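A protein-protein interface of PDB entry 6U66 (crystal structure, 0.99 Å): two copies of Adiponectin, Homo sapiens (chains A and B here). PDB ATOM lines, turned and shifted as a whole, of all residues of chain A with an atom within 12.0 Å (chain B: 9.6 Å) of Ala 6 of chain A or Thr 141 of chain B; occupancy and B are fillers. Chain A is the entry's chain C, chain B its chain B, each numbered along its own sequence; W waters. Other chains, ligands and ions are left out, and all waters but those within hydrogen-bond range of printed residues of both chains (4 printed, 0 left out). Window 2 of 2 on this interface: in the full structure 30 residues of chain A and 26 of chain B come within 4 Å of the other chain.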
ATOM      1  N   ALA A   6      -7.034   1.027  -1.802  1.00  0.00           N
ATOM      2  CA  ALA A   6      -8.280   0.333  -2.107  1.00  0.00           C
ATOM      3  C   ALA A   6      -8.571  -0.697  -1.021  1.00  0.00           C
ATOM      4  O   ALA A   6      -8.184  -1.863  -1.150  1.00  0.00           O
ATOM      5  CB  ALA A   6      -8.196  -0.356  -3.469  1.00  0.00           C
ATOM      6  N   TYR A   7      -9.239  -0.269   0.045  1.00  0.00           N
ATOM      7  CA  TYR A   7      -9.511  -1.148   1.180  1.00  0.00           C
ATOM      8  C   TYR A   7     -10.882  -1.815   1.021  1.00  0.00           C
ATOM      9  O   TYR A   7     -11.863  -1.173   0.631  1.00  0.00           O
ATOM     10  CB  TYR A   7      -9.455  -0.351   2.484  1.00  0.00           C
ATOM     11  CG  TYR A   7      -9.627  -1.191   3.694  1.00  0.00           C
ATOM     12  CD1 TYR A   7      -8.555  -1.871   4.262  1.00  0.00           C
ATOM     13  CD2 TYR A   7     -10.876  -1.338   4.266  1.00  0.00           C
ATOM     14  CE1 TYR A   7      -8.740  -2.677   5.365  1.00  0.00           C
ATOM     15  CE2 TYR A   7     -11.071  -2.131   5.366  1.00  0.00           C
ATOM     16  CZ  TYR A   7      -9.994  -2.813   5.909  1.00  0.00           C
ATOM     17  OH  TYR A   7     -10.217  -3.600   7.002  1.00  0.00           O
ATOM     18  N   VAL A   8     -10.932  -3.117   1.314  1.00  0.00           N
ATOM     19  CA  VAL A   8     -12.166  -3.884   1.304  1.00  0.00           C
ATOM     20  C   VAL A   8     -12.424  -4.343   2.723  1.00  0.00           C
ATOM     21  O   VAL A   8     -11.542  -4.931   3.354  1.00  0.00           O
ATOM     22  CB  VAL A   8     -12.055  -5.089   0.361  1.00  0.00           C
ATOM     23  CG1 VAL A   8     -13.315  -5.909   0.399  1.00  0.00           C
ATOM     24  CG2 VAL A   8     -11.761  -4.634  -1.096  1.00  0.00           C
ATOM     25  N   TYR A   9     -13.632  -4.113   3.202  1.00  0.00           N
ATOM     26  CA  TYR A   9     -14.081  -4.641   4.485  1.00  0.00           C
ATOM     27  C   TYR A   9     -14.523  -6.098   4.311  1.00  0.00           C
ATOM     28  O   TYR A   9     -15.512  -6.375   3.617  1.00  0.00           O
ATOM     29  CB  TYR A   9     -15.239  -3.834   5.066  1.00  0.00           C
ATOM     30  CG  TYR A   9     -14.845  -2.460   5.553  1.00  0.00           C
ATOM     31  CD1 TYR A   9     -14.617  -2.219   6.908  1.00  0.00           C
ATOM     32  CD2 TYR A   9     -14.681  -1.392   4.666  1.00  0.00           C
ATOM     33  CE1 TYR A   9     -14.249  -0.943   7.365  1.00  0.00           C
ATOM     34  CE2 TYR A   9     -14.298  -0.142   5.129  1.00  0.00           C
ATOM     35  CZ  TYR A   9     -14.080   0.049   6.473  1.00  0.00           C
ATOM     36  OH  TYR A   9     -13.740   1.320   6.936  1.00  0.00           O
ATOM     37  N   ARG A  10     -13.801  -7.029   4.940  1.00  0.00           N
ATOM     38  CA  ARG A  10     -14.066  -8.465   4.786  1.00  0.00           C
ATOM     39  C   ARG A  10     -14.407  -9.098   6.133  1.00  0.00           C
ATOM     40  O   ARG A  10     -13.644  -8.948   7.081  1.00  0.00           O
ATOM     41  CB  ARG A  10     -12.837  -9.200   4.238  1.00  0.00           C
ATOM     42  CG  ARG A  10     -12.322  -8.702   2.917  1.00  0.00           C
ATOM     43  CD  ARG A  10     -11.138  -9.548   2.438  1.00  0.00           C
ATOM     44  NE  ARG A  10     -10.530  -9.014   1.205  1.00  0.00           N
ATOM     45  CZ  ARG A  10      -9.739  -7.947   1.163  1.00  0.00           C
ATOM     46  NH1 ARG A  10      -9.324  -7.344   2.274  1.00  0.00           N
ATOM     47  NH2 ARG A  10      -9.307  -7.503   0.005  1.00  0.00           N
ATOM     48  N   SER A  11     -15.494  -9.864   6.190  1.00  0.00           N
ATOM     49  CA  SER A  11     -15.741 -10.730   7.326  1.00  0.00           C
ATOM     50  C   SER A  11     -16.652 -11.837   6.813  1.00  0.00           C
ATOM     51  O   SER A  11     -17.810 -11.591   6.493  1.00  0.00           O
ATOM     52  CB  SER A  11     -16.424  -9.992   8.480  1.00  0.00           C
ATOM     53  OG  SER A  11     -16.709 -10.945   9.500  1.00  0.00           O
ATOM     54  N   TYR A  35     -13.734 -21.536   4.141  1.00  0.00           N
ATOM     55  CA  TYR A  35     -13.139 -20.221   4.292  1.00  0.00           C
ATOM     56  C   TYR A  35     -13.383 -19.732   5.709  1.00  0.00           C
ATOM     57  O   TYR A  35     -14.485 -19.817   6.217  1.00  0.00           O
ATOM     58  CB  TYR A  35     -13.721 -19.239   3.285  1.00  0.00           C
ATOM     59  CG  TYR A  35     -13.127 -17.828   3.333  1.00  0.00           C
ATOM     60  CD1 TYR A  35     -12.088 -17.489   2.497  1.00  0.00           C
ATOM     61  CD2 TYR A  35     -13.654 -16.826   4.170  1.00  0.00           C
ATOM     62  CE1 TYR A  35     -11.555 -16.219   2.497  1.00  0.00           C
ATOM     63  CE2 TYR A  35     -13.127 -15.520   4.172  1.00  0.00           C
ATOM     64  CZ  TYR A  35     -12.100 -15.218   3.317  1.00  0.00           C
ATOM     65  OH  TYR A  35     -11.628 -13.911   3.278  1.00  0.00           O
ATOM     66  N   GLN A  37     -11.011 -16.723   6.886  1.00  0.00           N
ATOM     67  CA  GLN A  37      -9.715 -16.052   6.905  1.00  0.00           C
ATOM     68  C   GLN A  37      -9.588 -15.029   8.022  1.00  0.00           C
ATOM     69  O   GLN A  37      -8.471 -14.747   8.466  1.00  0.00           O
ATOM     70  CB  GLN A  37      -9.474 -15.391   5.549  1.00  0.00           C
ATOM     71  CG  GLN A  37      -8.206 -14.649   5.421  1.00  0.00           C
ATOM     72  CD  GLN A  37      -8.005 -14.169   4.024  1.00  0.00           C
ATOM     73  OE1 GLN A  37      -7.978 -14.964   3.088  1.00  0.00           O
ATOM     74  NE2 GLN A  37      -7.907 -12.834   3.856  1.00  0.00           N
ATOM     75  N   GLN A  38     -10.711 -14.442   8.478  1.00  0.00           N
ATOM     76  CA  GLN A  38     -10.672 -13.456   9.546  1.00  0.00           C
ATOM     77  C   GLN A  38     -10.762 -14.104  10.920  1.00  0.00           C
ATOM     78  O   GLN A  38     -10.654 -13.395  11.935  1.00  0.00           O
ATOM     79  CB  GLN A  38     -11.806 -12.424   9.372  1.00  0.00           C
ATOM     80  CG  GLN A  38     -11.675 -11.622   8.098  1.00  0.00           C
ATOM     81  CD  GLN A  38     -12.179 -12.362   6.879  1.00  0.00           C
ATOM     82  OE1 GLN A  38     -13.189 -13.058   6.929  1.00  0.00           O
ATOM     83  NE2 GLN A  38     -11.458 -12.238   5.768  1.00  0.00           N
ATOM     84  N   HIS A 139     -20.749  -2.915   4.979  1.00  0.00           N
ATOM     85  CA  HIS A 139     -20.352  -2.356   6.267  1.00  0.00           C
ATOM     86  C   HIS A 139     -21.131  -1.060   6.517  1.00  0.00           C
ATOM     87  O   HIS A 139     -21.387  -0.301   5.597  1.00  0.00           O
ATOM     88  CB  HIS A 139     -18.827  -2.123   6.340  1.00  0.00           C
ATOM     89  CG  HIS A 139     -18.302  -0.965   5.543  1.00  0.00           C
ATOM     90  ND1 HIS A 139     -18.121  -1.019   4.182  1.00  0.00           N
ATOM     91  CD2 HIS A 139     -17.840   0.247   5.935  1.00  0.00           C
ATOM     92  CE1 HIS A 139     -17.584   0.114   3.769  1.00  0.00           C
ATOM     93  NE2 HIS A 139     -17.414   0.899   4.799  1.00  0.00           N
ATOM     94  N   ALA B   6     -15.533   5.220  -7.269  1.00  0.00           N
ATOM     95  CA  ALA B   6     -14.716   4.035  -7.054  1.00  0.00           C
ATOM     96  C   ALA B   6     -14.958   3.018  -8.155  1.00  0.00           C
ATOM     97  O   ALA B   6     -16.100   2.748  -8.533  1.00  0.00           O
ATOM     98  CB  ALA B   6     -15.091   3.439  -5.699  1.00  0.00           C
ATOM     99  N   TYR B   7     -13.866   2.428  -8.650  1.00  0.00           N
ATOM    100  CA  TYR B   7     -13.959   1.350  -9.643  1.00  0.00           C
ATOM    101  C   TYR B   7     -14.657   0.127  -9.044  1.00  0.00           C
ATOM    102  O   TYR B   7     -14.412  -0.270  -7.900  1.00  0.00           O
ATOM    103  CB  TYR B   7     -12.525   0.971 -10.071  1.00  0.00           C
ATOM    104  CG  TYR B   7     -12.466   0.033 -11.238  1.00  0.00           C
ATOM    105  CD1 TYR B   7     -12.376   0.489 -12.554  1.00  0.00           C
ATOM    106  CD2 TYR B   7     -12.481  -1.351 -11.057  1.00  0.00           C
ATOM    107  CE1 TYR B   7     -12.306  -0.388 -13.615  1.00  0.00           C
ATOM    108  CE2 TYR B   7     -12.416  -2.242 -12.120  1.00  0.00           C
ATOM    109  CZ  TYR B   7     -12.363  -1.740 -13.399  1.00  0.00           C
ATOM    110  OH  TYR B   7     -12.274  -2.563 -14.482  1.00  0.00           O
ATOM    111  N   TYR B   9     -15.298  -3.868  -9.295  1.00  0.00           N
ATOM    112  CA  TYR B   9     -14.797  -5.160  -9.766  1.00  0.00           C
ATOM    113  C   TYR B   9     -15.946  -6.162  -9.849  1.00  0.00           C
ATOM    114  O   TYR B   9     -16.509  -6.520  -8.819  1.00  0.00           O
ATOM    115  CB  TYR B   9     -13.711  -5.698  -8.825  1.00  0.00           C
ATOM    116  CG  TYR B   9     -12.440  -4.861  -8.864  1.00  0.00           C
ATOM    117  CD1 TYR B   9     -11.463  -5.129  -9.802  1.00  0.00           C
ATOM    118  CD2 TYR B   9     -12.248  -3.801  -8.017  1.00  0.00           C
ATOM    119  CE1 TYR B   9     -10.325  -4.334  -9.877  1.00  0.00           C
ATOM    120  CE2 TYR B   9     -11.141  -3.016  -8.094  1.00  0.00           C
ATOM    121  CZ  TYR B   9     -10.178  -3.281  -9.016  1.00  0.00           C
ATOM    122  OH  TYR B   9      -9.050  -2.482  -9.080  1.00  0.00           O
ATOM    123  N   ILE B  52     -10.211 -12.543 -11.595  1.00  0.00           N
ATOM    124  CA  ILE B  52      -9.915 -11.537 -10.578  1.00  0.00           C
ATOM    125  C   ILE B  52      -9.729 -12.325  -9.288  1.00  0.00           C
ATOM    126  O   ILE B  52     -10.675 -12.955  -8.817  1.00  0.00           O
ATOM    127  CB  ILE B  52     -11.059 -10.525 -10.387  1.00  0.00           C
ATOM    128  CG1 ILE B  52     -11.366  -9.768 -11.680  1.00  0.00           C
ATOM    129  CG2 ILE B  52     -10.763  -9.594  -9.208  1.00  0.00           C
ATOM    130  CD1 ILE B  52     -12.651  -8.948 -11.593  1.00  0.00           C
ATOM    131  N   PRO B  53      -8.560 -12.311  -8.662  1.00  0.00           N
ATOM    132  CA  PRO B  53      -8.395 -13.114  -7.432  1.00  0.00           C
ATOM    133  C   PRO B  53      -9.244 -12.531  -6.304  1.00  0.00           C
ATOM    134  O   PRO B  53      -9.377 -11.318  -6.155  1.00  0.00           O
ATOM    135  CB  PRO B  53      -6.890 -13.044  -7.156  1.00  0.00           C
ATOM    136  CG  PRO B  53      -6.506 -11.708  -7.756  1.00  0.00           C
ATOM    137  CD  PRO B  53      -7.362 -11.513  -8.944  1.00  0.00           C
ATOM    138  N   GLY B  54      -9.831 -13.414  -5.503  1.00  0.00           N
ATOM    139  CA  GLY B  54     -10.699 -12.958  -4.433  1.00  0.00           C
ATOM    140  C   GLY B  54     -11.597 -14.057  -3.899  1.00  0.00           C
ATOM    141  O   GLY B  54     -11.448 -15.249  -4.206  1.00  0.00           O
ATOM    142  N   LEU B  55     -12.541 -13.638  -3.074  1.00  0.00           N
ATOM    143  CA  LEU B  55     -13.487 -14.538  -2.412  1.00  0.00           C
ATOM    144  C   LEU B  55     -14.761 -14.565  -3.232  1.00  0.00           C
ATOM    145  O   LEU B  55     -15.343 -13.509  -3.513  1.00  0.00           O
ATOM    146  CB  LEU B  55     -13.800 -14.066  -1.000  1.00  0.00           C
ATOM    147  CG  LEU B  55     -14.709 -14.988  -0.203  1.00  0.00           C
ATOM    148  CD1 LEU B  55     -14.074 -16.354  -0.060  1.00  0.00           C
ATOM    149  CD2 LEU B  55     -15.048 -14.363   1.184  1.00  0.00           C
ATOM    150  N   HIS B 102     -12.180 -19.064  -1.830  1.00  0.00           N
ATOM    151  CA  HIS B 102     -11.182 -18.142  -2.330  1.00  0.00           C
ATOM    152  C   HIS B 102     -10.556 -18.705  -3.609  1.00  0.00           C
ATOM    153  O   HIS B 102     -10.187 -19.895  -3.644  1.00  0.00           O
ATOM    154  CB  HIS B 102     -10.101 -17.853  -1.317  1.00  0.00           C
ATOM    155  CG  HIS B 102      -9.198 -16.763  -1.758  1.00  0.00           C
ATOM    156  ND1 HIS B 102      -8.100 -16.965  -2.569  1.00  0.00           N
ATOM    157  CD2 HIS B 102      -9.301 -15.423  -1.585  1.00  0.00           C
ATOM    158  CE1 HIS B 102      -7.548 -15.784  -2.830  1.00  0.00           C
ATOM    159  NE2 HIS B 102      -8.263 -14.844  -2.261  1.00  0.00           N
ATOM    160  N   GLU B 104      -7.746 -17.981  -7.009  1.00  0.00           N
ATOM    161  CA  GLU B 104      -6.663 -17.293  -7.707  1.00  0.00           C
ATOM    162  C   GLU B 104      -6.931 -17.295  -9.210  1.00  0.00           C
ATOM    163  O   GLU B 104      -7.729 -18.095  -9.736  1.00  0.00           O
ATOM    164  CB  GLU B 104      -5.317 -17.969  -7.431  1.00  0.00           C
ATOM    165  CG  GLU B 104      -4.931 -18.030  -5.948  1.00  0.00           C
ATOM    166  CD  GLU B 104      -4.596 -16.663  -5.318  1.00  0.00           C
ATOM    167  OE1 GLU B 104      -4.382 -15.674  -6.048  1.00  0.00           O
ATOM    168  OE2 GLU B 104      -4.568 -16.573  -4.066  1.00  0.00           O
ATOM    169  N   LEU B 136     -18.004 -12.882  -7.576  1.00  0.00           N
ATOM    170  CA  LEU B 136     -16.963 -12.258  -6.777  1.00  0.00           C
ATOM    171  C   LEU B 136     -17.596 -11.406  -5.685  1.00  0.00           C
ATOM    172  O   LEU B 136     -18.372 -10.478  -5.952  1.00  0.00           O
ATOM    173  CB  LEU B 136     -16.090 -11.370  -7.669  1.00  0.00           C
ATOM    174  CG  LEU B 136     -15.054 -10.514  -6.956  1.00  0.00           C
ATOM    175  CD1 LEU B 136     -13.949 -11.328  -6.298  1.00  0.00           C
ATOM    176  CD2 LEU B 136     -14.444  -9.545  -7.931  1.00  0.00           C
ATOM    177  N   TYR B 138     -15.418 -10.380  -2.602  1.00  0.00           N
ATOM    178  CA  TYR B 138     -14.335  -9.496  -2.169  1.00  0.00           C
ATOM    179  C   TYR B 138     -13.103  -9.694  -3.063  1.00  0.00           C
ATOM    180  O   TYR B 138     -12.452 -10.739  -3.007  1.00  0.00           O
ATOM    181  CB  TYR B 138     -13.871  -9.780  -0.739  1.00  0.00           C
ATOM    182  CG  TYR B 138     -14.896  -9.813   0.366  1.00  0.00           C
ATOM    183  CD1 TYR B 138     -15.912  -8.881   0.489  1.00  0.00           C
ATOM    184  CD2 TYR B 138     -14.799 -10.771   1.357  1.00  0.00           C
ATOM    185  CE1 TYR B 138     -16.822  -8.922   1.525  1.00  0.00           C
ATOM    186  CE2 TYR B 138     -15.661 -10.847   2.412  1.00  0.00           C
ATOM    187  CZ  TYR B 138     -16.700  -9.917   2.511  1.00  0.00           C
ATOM    188  OH  TYR B 138     -17.557 -10.022   3.580  1.00  0.00           O
ATOM    189  N   HIS B 139     -12.745  -8.702  -3.874  1.00  0.00           N
ATOM    190  CA  HIS B 139     -11.491  -8.790  -4.584  1.00  0.00           C
ATOM    191  C   HIS B 139     -10.326  -8.714  -3.607  1.00  0.00           C
ATOM    192  O   HIS B 139     -10.391  -8.006  -2.603  1.00  0.00           O
ATOM    193  CB  HIS B 139     -11.387  -7.733  -5.698  1.00  0.00           C
ATOM    194  CG  HIS B 139     -11.065  -6.354  -5.259  1.00  0.00           C
ATOM    195  ND1 HIS B 139     -12.006  -5.433  -4.849  1.00  0.00           N
ATOM    196  CD2 HIS B 139      -9.887  -5.693  -5.284  1.00  0.00           C
ATOM    197  CE1 HIS B 139     -11.403  -4.287  -4.549  1.00  0.00           C
ATOM    198  NE2 HIS B 139     -10.119  -4.421  -4.810  1.00  0.00           N
ATOM    199  N   ASP B 140      -9.272  -9.452  -3.912  1.00  0.00           N
ATOM    200  CA  ASP B 140      -8.052  -9.373  -3.108  1.00  0.00           C
ATOM    201  C   ASP B 140      -7.387  -8.009  -3.289  1.00  0.00           C
ATOM    202  O   ASP B 140      -7.450  -7.389  -4.368  1.00  0.00           O
ATOM    203  CB  ASP B 140      -7.038 -10.452  -3.520  1.00  0.00           C
ATOM    204  CG  ASP B 140      -7.385 -11.856  -3.019  1.00  0.00           C
ATOM    205  OD1 ASP B 140      -8.300 -12.011  -2.219  1.00  0.00           O
ATOM    206  OD2 ASP B 140      -6.697 -12.791  -3.462  1.00  0.00           O
ATOM    207  N   THR B 141      -6.723  -7.557  -2.231  1.00  0.00           N
ATOM    208  CA  THR B 141      -5.927  -6.335  -2.286  1.00  0.00           C
ATOM    209  C   THR B 141      -4.553  -6.652  -1.709  1.00  0.00           C
ATOM    210  O   THR B 141      -4.380  -7.573  -0.914  1.00  0.00           O
ATOM    211  CB  THR B 141      -6.630  -5.194  -1.552  1.00  0.00           C
ATOM    212  OG1 THR B 141      -6.995  -5.597  -0.247  1.00  0.00           O
ATOM    213  CG2 THR B 141      -7.894  -4.788  -2.303  1.00  0.00           C
ATOM    214  N   ASN B 142      -3.560  -5.901  -2.125  1.00  0.00           N
ATOM    215  CA  ASN B 142      -2.196  -6.269  -1.731  1.00  0.00           C
ATOM    216  C   ASN B 142      -1.295  -5.085  -1.904  1.00  0.00           C
ATOM    217  O   ASN B 142      -1.276  -4.525  -3.009  1.00  0.00           O
ATOM    218  CB  ASN B 142      -1.691  -7.435  -2.594  1.00  0.00           C
ATOM    219  OXT ASN B 142      -0.595  -4.692  -0.959  1.00  0.00           O
HETATM  220  O   HOH W   1      -7.682 -12.886   0.798  1.00  0.00           O
HETATM  221  O   HOH W   2     -10.540 -11.085  -0.900  1.00  0.00           O
HETATM  222  O   HOH W   3      -8.419  -4.642   2.130  1.00  0.00           O
HETATM  223  O   HOH W   4      -6.478  -9.531  -0.014  1.00  0.00           O
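Ala 6 of chain A touches one residue of chain B. Thr 141 of chain B touches just these residues of chain A: Ala 6 (3.2 Å) and Arg 10 (3.0 Å). Of chain A, only Val 8 and Arg 10 come within 4 Å of His 139 of chain B. Printed residues of chain A within 4 Å of Asp 140 of chain B: Arg 10 (3.8 Å). No residue of chain A comes within 4 Å of Asn 142 of chain B. Printed residues of chain A within 4 Å of Leu 55 of chain B: Tyr 35. Printed residues of chain A within 4 Å of Tyr 138 of chain B: Val 8 (3.9 Å), Tyr 9 (3.5 Å), Arg 10 (3.6 Å) and Ser 11 (3.3 Å). Of the printed residues of chain B, Val 8 of chain A touches Tyr 138 (3.9 Å) and His 139 (3.5 Å). Of the printed residues of chain B, Arg 10 of chain A touches Tyr 138, His 139, Asp 140 and Thr 141. Of the printed residues of chain B, Ser 11 of chain A touches Tyr 138 (3.3 Å). Ala 6 of chain B touches none of the printed residues of chain A. The nearest printed residue of chain B that does not touch Val 8 of chain A is Thr 141 of chain B (4.1 Å).
O of Pro 53 of chain B lies within hydrogen-bond range of N of Asp 140 of chain B (2.9 Å). O of Tyr 138 of chain B is in hydrogen-bond range of N of Leu 55 of chain B, 2.9 Å away. A ring nitrogen (NE2) of His 102 of chain B lies within hydrogen-bond range of the side-chain carboxylate (OD1) of Asp 140 of chain B (2.8 Å). O of Val 8 of chain A sits at hydrogen-bond distance from NH1 of Arg 10 of chain A, 3.5 Å away. OH of Tyr 35 of chain A sits at hydrogen-bond distance from NE2 of Gln 38 of chain A, 3.0 Å away.
Water W2 lies within hydrogen-bond range of OD1 of Asp 140 of chain B (2.8 Å), O of Tyr 138 of chain B (2.9 Å) and NE of Arg 10 of chain A (3.0 Å). Water W3 lies within hydrogen-bond range of the guanidinium group of Arg 10 of chain A (2.9 Å), the side-chain hydroxyl of Thr 141 of chain B (2.9 Å) and the backbone NH of Val 8 of chain A (3.1 Å). Water W4 lies within hydrogen-bond range of N of Thr 141 of chain B (3.0 Å) and NH2 of Arg 10 of chain A (3.5 Å). Water W1 bridges the side-chain amide nitrogen of Gln 37 of chain A and the side-chain carboxylate of Asp 140 of chain B.
The side-chain hydroxyl (OH) of Tyr 138 of chain B sits at hydrogen-bond distance from the backbone carbonyl oxygen (O) of Ser 11 of chain A, at 3.3 Å. O of His 139 of chain B lies within hydrogen-bond range of NH2 of Arg 10 of chain A, at 2.9 Å. OG1 of Thr 141 of chain B lies within hydrogen-bond range of NH2 of Arg 10 of chain A (3.0 Å).
Of the 15 printed residues of chain B, 5 touch a printed residue of chain A. Among the printed residues, 10 pairs touch across the chains.
Ala 6 of chain A touches Thr 141 of chain B. CD1 of Tyr 138 of chain B touches CG1 of Val 8 of chain A, 3.9 Å away. CG2 of Val 8 of chain A touches CE1 of His 139 of chain B, 3.5 Å away. Tyr 138 of chain B touches Tyr 9 of chain A. Arg 10 of chain A touches Tyr 138 of chain B. Asp 140 of chain B touches Arg 10 of chain A. CD1 of Tyr 35 of chain A touches CD1 of Leu 55 of chain B, at 3.4 Å.
4 positions are printed for both chains.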
